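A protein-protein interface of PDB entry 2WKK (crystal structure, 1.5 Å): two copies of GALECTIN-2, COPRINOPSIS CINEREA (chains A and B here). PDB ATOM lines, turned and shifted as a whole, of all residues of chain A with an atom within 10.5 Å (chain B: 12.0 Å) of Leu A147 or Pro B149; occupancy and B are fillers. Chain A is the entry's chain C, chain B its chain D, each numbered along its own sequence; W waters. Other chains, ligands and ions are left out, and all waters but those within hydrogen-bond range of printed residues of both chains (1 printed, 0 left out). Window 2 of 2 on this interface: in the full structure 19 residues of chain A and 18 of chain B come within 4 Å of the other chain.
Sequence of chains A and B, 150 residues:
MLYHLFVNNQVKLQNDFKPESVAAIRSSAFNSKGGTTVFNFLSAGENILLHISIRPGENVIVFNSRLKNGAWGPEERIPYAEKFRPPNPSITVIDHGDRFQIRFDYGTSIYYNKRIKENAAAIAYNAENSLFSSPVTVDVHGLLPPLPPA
Pro A146 touches Pro B148. Pro A146 touches Pro B149 (CB to O, 3.9 Å). Pro B148 touches Leu A147. Pro B149 touches Leu A147. Pro A148 touches Pro B146 (CB to O, 3.6 Å). Leu B147 touches Pro A148. Pro A148 touches Pro B148. Pro B146 touches Pro A149 (CB to CD, 3.9 Å). O of Leu B147 touches CD of Pro A149, 3.1 Å away. Ala A150 touches Pro B146.
Of the printed residues of chain B, Leu A147 touches Pro B148 (3.8 Å) and Pro B149 (3.1 Å). Of the printed residues of chain A, Pro B149 touches Pro A146 (3.9 Å) and Leu A147 (3.1 Å). No residue of chain B comes within 4 Å of Pro A145. Of chain B, only Pro B146 (3.6 Å), Leu B147 (3.7 Å) and Pro B148 (3.8 Å) come within 4 Å of Pro A148. Of chain A, only Pro A146 (3.6 Å), Leu A147 (3.8 Å) and Pro A148 (3.8 Å) come within 4 Å of Pro B148. Of the printed residues of chain B, Pro A146 touches Pro B148 (3.6 Å) and Pro B149 (3.9 Å). Of the printed residues of chain A, Leu B147 touches Pro A148 and Pro A149. Printed residues of chain B within 4 Å of Ala A150: Pro B146 (3.9 Å). His A141 touches none of the printed residues of chain B. The nearest printed residue of chain B that does not touch Leu A147 is Leu B147 (4.7 Å).
Of the 12 printed residues of chain A, 5 touch a printed residue of chain B. Printed residues of chain A that touch a printed residue of chain B: Pro A146, Leu A147, Pro A148, Pro A149 and Ala A150. Hydrophobic or aromatic side chains of chain A that line the printed part of chain B: Pro A146, Pro A148 and Pro A149. Of the 7 printed residues of chain B, 4 touch a printed residue of chain A. Printed residues of chain B that touch a printed residue of chain A: Pro B146, Leu B147, Pro B148 and Pro B149. Hydrophobic or aromatic side chains of chain B within 4 Å of the printed part of chain A: Pro B146, Pro B148 and Pro B149. Among the printed residues, 10 pairs touch across the chains.
Pro A146 touches Pro B148, and with the chains exchanged Pro A148 touches Pro B146. Leu A147 touches Pro B149, and with the chains exchanged Pro A149 touches Leu B147. Pro B148 touches its own counterpart, Pro A148. Ala A150 touches Pro B146, but with the chains exchanged Pro A146 does not touch Ala B150 (4.8 Å). 7 positions are printed for both chains. Of the 10 pairs that touch across the chains among the printed residues, 9 have their exchanged pair printed and touching as well.
Water W1 lies within hydrogen-bond range of O of Pro B146 and O of Ala A150.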
ATOM      1  N   VAL A  22     -29.606   1.187  26.101  1.00  0.00           N
ATOM      2  CA  VAL A  22     -28.199   0.831  26.103  1.00  0.00           C
ATOM      3  C   VAL A  22     -27.627   1.149  27.482  1.00  0.00           C
ATOM      4  O   VAL A  22     -27.803   2.260  27.984  1.00  0.00           O
ATOM      5  CB  VAL A  22     -27.421   1.652  25.035  1.00  0.00           C
ATOM      6  CG1 VAL A  22     -25.940   1.303  25.056  1.00  0.00           C
ATOM      7  CG2 VAL A  22     -28.012   1.411  23.638  1.00  0.00           C
ATOM      8  N   THR A  92     -21.144  -3.750  27.949  1.00  0.00           N
ATOM      9  CA  THR A  92     -22.201  -2.975  27.320  1.00  0.00           C
ATOM     10  C   THR A  92     -23.390  -3.888  27.053  1.00  0.00           C
ATOM     11  O   THR A  92     -23.245  -4.948  26.433  1.00  0.00           O
ATOM     12  CB  THR A  92     -21.704  -2.302  26.024  1.00  0.00           C
ATOM     13  OG1 THR A  92     -20.584  -1.458  26.338  1.00  0.00           O
ATOM     14  CG2 THR A  92     -22.804  -1.450  25.394  1.00  0.00           C
ATOM     15  N   ILE A  94     -27.341  -4.112  25.552  1.00  0.00           N
ATOM     16  CA  ILE A  94     -28.331  -3.467  24.702  1.00  0.00           C
ATOM     17  C   ILE A  94     -29.573  -4.352  24.602  1.00  0.00           C
ATOM     18  O   ILE A  94     -29.479  -5.564  24.389  1.00  0.00           O
ATOM     19  CB  ILE A  94     -27.752  -3.140  23.295  1.00  0.00           C
ATOM     20  CG1 ILE A  94     -26.542  -2.210  23.437  1.00  0.00           C
ATOM     21  CG2 ILE A  94     -28.819  -2.495  22.388  1.00  0.00           C
ATOM     22  CD1 ILE A  94     -25.840  -1.867  22.122  1.00  0.00           C
ATOM     23  N   HIS A 141     -28.833   4.850  28.154  1.00  0.00           N
ATOM     24  CA  HIS A 141     -29.477   5.589  27.067  1.00  0.00           C
ATOM     25  C   HIS A 141     -30.808   4.935  26.732  1.00  0.00           C
ATOM     26  O   HIS A 141     -30.935   3.719  26.835  1.00  0.00           O
ATOM     27  CB  HIS A 141     -28.619   5.519  25.805  1.00  0.00           C
ATOM     28  CG  HIS A 141     -27.200   5.947  26.003  1.00  0.00           C
ATOM     29  ND1 HIS A 141     -26.713   7.146  25.530  1.00  0.00           N
ATOM     30  CD2 HIS A 141     -26.156   5.326  26.603  1.00  0.00           C
ATOM     31  CE1 HIS A 141     -25.433   7.250  25.842  1.00  0.00           C
ATOM     32  NE2 HIS A 141     -25.072   6.160  26.496  1.00  0.00           N
ATOM     33  N   LEU A 143     -31.926   5.179  23.696  1.00  0.00           N
ATOM     34  CA  LEU A 143     -31.633   4.731  22.342  1.00  0.00           C
ATOM     35  C   LEU A 143     -30.159   4.977  22.049  1.00  0.00           C
ATOM     36  O   LEU A 143     -29.497   5.784  22.724  1.00  0.00           O
ATOM     37  CB  LEU A 143     -32.513   5.448  21.314  1.00  0.00           C
ATOM     38  CG  LEU A 143     -32.115   6.865  20.908  1.00  0.00           C
ATOM     39  CD1 LEU A 143     -32.870   7.300  19.654  1.00  0.00           C
ATOM     40  CD2 LEU A 143     -32.344   7.838  22.052  1.00  0.00           C
ATOM     41  N   LEU A 144     -29.634   4.264  21.063  1.00  0.00           N
ATOM     42  CA  LEU A 144     -28.229   4.397  20.704  1.00  0.00           C
ATOM     43  C   LEU A 144     -27.922   5.850  20.333  1.00  0.00           C
ATOM     44  O   LEU A 144     -28.623   6.439  19.509  1.00  0.00           O
ATOM     45  CB  LEU A 144     -27.903   3.484  19.523  1.00  0.00           C
ATOM     46  CG  LEU A 144     -26.421   3.286  19.217  1.00  0.00           C
ATOM     47  CD1 LEU A 144     -25.756   2.459  20.322  1.00  0.00           C
ATOM     48  CD2 LEU A 144     -26.254   2.616  17.852  1.00  0.00           C
ATOM     49  N   PRO A 145     -26.886   6.444  20.951  1.00  0.00           N
ATOM     50  CA  PRO A 145     -26.554   7.843  20.651  1.00  0.00           C
ATOM     51  C   PRO A 145     -25.851   7.975  19.307  1.00  0.00           C
ATOM     52  O   PRO A 145     -25.354   6.978  18.782  1.00  0.00           O
ATOM     53  CB  PRO A 145     -25.561   8.202  21.763  1.00  0.00           C
ATOM     54  CG  PRO A 145     -24.905   6.888  22.077  1.00  0.00           C
ATOM     55  CD  PRO A 145     -26.053   5.909  22.042  1.00  0.00           C
ATOM     56  N   PRO A 146     -25.795   9.198  18.761  1.00  0.00           N
ATOM     57  CA  PRO A 146     -24.958   9.466  17.590  1.00  0.00           C
ATOM     58  C   PRO A 146     -23.536   8.999  17.858  1.00  0.00           C
ATOM     59  O   PRO A 146     -23.025   9.182  18.969  1.00  0.00           O
ATOM     60  CB  PRO A 146     -25.014  10.988  17.464  1.00  0.00           C
ATOM     61  CG  PRO A 146     -26.351  11.336  18.012  1.00  0.00           C
ATOM     62  CD  PRO A 146     -26.544  10.394  19.180  1.00  0.00           C
ATOM     63  N   LEU A 147     -22.910   8.394  16.853  1.00  0.00           N
ATOM     64  CA  LEU A 147     -21.609   7.764  17.041  1.00  0.00           C
ATOM     65  C   LEU A 147     -20.453   8.626  16.548  1.00  0.00           C
ATOM     66  O   LEU A 147     -20.515   9.203  15.467  1.00  0.00           O
ATOM     67  CB  LEU A 147     -21.571   6.423  16.308  1.00  0.00           C
ATOM     68  CG  LEU A 147     -22.656   5.422  16.676  1.00  0.00           C
ATOM     69  CD1 LEU A 147     -22.551   4.190  15.780  1.00  0.00           C
ATOM     70  CD2 LEU A 147     -22.559   5.046  18.141  1.00  0.00           C
ATOM     71  N   PRO A 148     -19.374   8.692  17.331  1.00  0.00           N
ATOM     72  CA  PRO A 148     -18.156   9.339  16.838  1.00  0.00           C
ATOM     73  C   PRO A 148     -17.585   8.530  15.673  1.00  0.00           C
ATOM     74  O   PRO A 148     -17.886   7.337  15.547  1.00  0.00           O
ATOM     75  CB  PRO A 148     -17.211   9.241  18.035  1.00  0.00           C
ATOM     76  CG  PRO A 148     -17.687   8.005  18.751  1.00  0.00           C
ATOM     77  CD  PRO A 148     -19.183   8.086  18.658  1.00  0.00           C
ATOM     78  N   PRO A 149     -16.772   9.164  14.823  1.00  0.00           N
ATOM     79  CA  PRO A 149     -16.110   8.430  13.739  1.00  0.00           C
ATOM     80  C   PRO A 149     -15.164   7.339  14.237  1.00  0.00           C
ATOM     81  O   PRO A 149     -14.834   6.420  13.481  1.00  0.00           O
ATOM     82  CB  PRO A 149     -15.300   9.508  13.013  1.00  0.00           C
ATOM     83  CG  PRO A 149     -15.844  10.806  13.450  1.00  0.00           C
ATOM     84  CD  PRO A 149     -16.494  10.611  14.784  1.00  0.00           C
ATOM     85  N   ALA A 150     -14.718   7.418  15.484  1.00  0.00           N
ATOM     86  CA  ALA A 150     -13.803   6.379  15.955  1.00  0.00           C
ATOM     87  C   ALA A 150     -13.746   6.270  17.471  1.00  0.00           C
ATOM     88  O   ALA A 150     -14.403   7.034  18.158  1.00  0.00           O
ATOM     89  CB  ALA A 150     -12.408   6.584  15.368  1.00  0.00           C
ATOM     90  OXT ALA A 150     -13.055   5.418  18.029  1.00  0.00           O
ATOM     91  N   LEU B 144      -8.283  15.784  22.241  1.00  0.00           N
ATOM     92  CA  LEU B 144      -9.713  15.779  21.952  1.00  0.00           C
ATOM     93  C   LEU B 144     -10.061  14.492  21.207  1.00  0.00           C
ATOM     94  O   LEU B 144      -9.432  14.181  20.194  1.00  0.00           O
ATOM     95  CB  LEU B 144     -10.052  16.975  21.059  1.00  0.00           C
ATOM     96  CG  LEU B 144     -11.134  18.003  21.401  1.00  0.00           C
ATOM     97  CD1 LEU B 144     -11.898  18.395  20.143  1.00  0.00           C
ATOM     98  CD2 LEU B 144     -12.068  17.545  22.490  1.00  0.00           C
ATOM     99  N   PRO B 145     -11.052  13.729  21.703  1.00  0.00           N
ATOM    100  CA  PRO B 145     -11.432  12.499  20.992  1.00  0.00           C
ATOM    101  C   PRO B 145     -12.250  12.812  19.740  1.00  0.00           C
ATOM    102  O   PRO B 145     -12.704  13.948  19.565  1.00  0.00           O
ATOM    103  CB  PRO B 145     -12.316  11.775  22.017  1.00  0.00           C
ATOM    104  CG  PRO B 145     -12.960  12.906  22.775  1.00  0.00           C
ATOM    105  CD  PRO B 145     -11.813  13.887  22.957  1.00  0.00           C
ATOM    106  N   PRO B 146     -12.447  11.812  18.871  1.00  0.00           N
ATOM    107  CA  PRO B 146     -13.332  12.042  17.726  1.00  0.00           C
ATOM    108  C   PRO B 146     -14.721  12.395  18.237  1.00  0.00           C
ATOM    109  O   PRO B 146     -15.143  11.859  19.268  1.00  0.00           O
ATOM    110  CB  PRO B 146     -13.354  10.686  17.017  1.00  0.00           C
ATOM    111  CG  PRO B 146     -12.075  10.015  17.439  1.00  0.00           C
ATOM    112  CD  PRO B 146     -11.838  10.473  18.854  1.00  0.00           C
ATOM    113  N   LEU B 147     -15.409  13.292  17.537  1.00  0.00           N
ATOM    114  CA  LEU B 147     -16.680  13.841  18.009  1.00  0.00           C
ATOM    115  C   LEU B 147     -17.881  13.205  17.326  1.00  0.00           C
ATOM    116  O   LEU B 147     -17.876  13.000  16.122  1.00  0.00           O
ATOM    117  CB  LEU B 147     -16.718  15.352  17.763  1.00  0.00           C
ATOM    118  CG  LEU B 147     -15.583  16.171  18.383  1.00  0.00           C
ATOM    119  CD1 LEU B 147     -15.685  17.634  17.960  1.00  0.00           C
ATOM    120  CD2 LEU B 147     -15.581  16.034  19.907  1.00  0.00           C
ATOM    121  N   PRO B 148     -18.935  12.926  18.098  1.00  0.00           N
ATOM    122  CA  PRO B 148     -20.182  12.460  17.490  1.00  0.00           C
ATOM    123  C   PRO B 148     -20.788  13.606  16.703  1.00  0.00           C
ATOM    124  O   PRO B 148     -20.451  14.764  16.955  1.00  0.00           O
ATOM    125  CB  PRO B 148     -21.061  12.155  18.710  1.00  0.00           C
ATOM    126  CG  PRO B 148     -20.519  13.092  19.770  1.00  0.00           C
ATOM    127  CD  PRO B 148     -19.034  13.008  19.564  1.00  0.00           C
ATOM    128  N   PRO B 149     -21.651  13.296  15.733  1.00  0.00           N
ATOM    129  CA  PRO B 149     -22.305  14.374  14.986  1.00  0.00           C
ATOM    130  C   PRO B 149     -23.472  14.963  15.772  1.00  0.00           C
ATOM    131  O   PRO B 149     -23.687  14.603  16.933  1.00  0.00           O
ATOM    132  CB  PRO B 149     -22.840  13.668  13.734  1.00  0.00           C
ATOM    133  CG  PRO B 149     -22.319  12.250  13.787  1.00  0.00           C
ATOM    134  CD  PRO B 149     -21.994  11.965  15.211  1.00  0.00           C
ATOM    135  N   ALA B 150     -24.201  15.868  15.124  1.00  0.00           N
ATOM    136  CA  ALA B 150     -25.454  16.425  15.636  1.00  0.00           C
ATOM    137  C   ALA B 150     -25.601  16.381  17.149  1.00  0.00           C
ATOM    138  O   ALA B 150     -24.662  16.660  17.894  1.00  0.00           O
ATOM    139  CB  ALA B 150     -26.644  15.741  14.969  1.00  0.00           C
ATOM    140  OXT ALA B 150     -26.679  16.078  17.657  1.00  0.00           O
HETATM  141  O   HOH W   1     -14.306   9.248  20.019  1.00  0.00           O
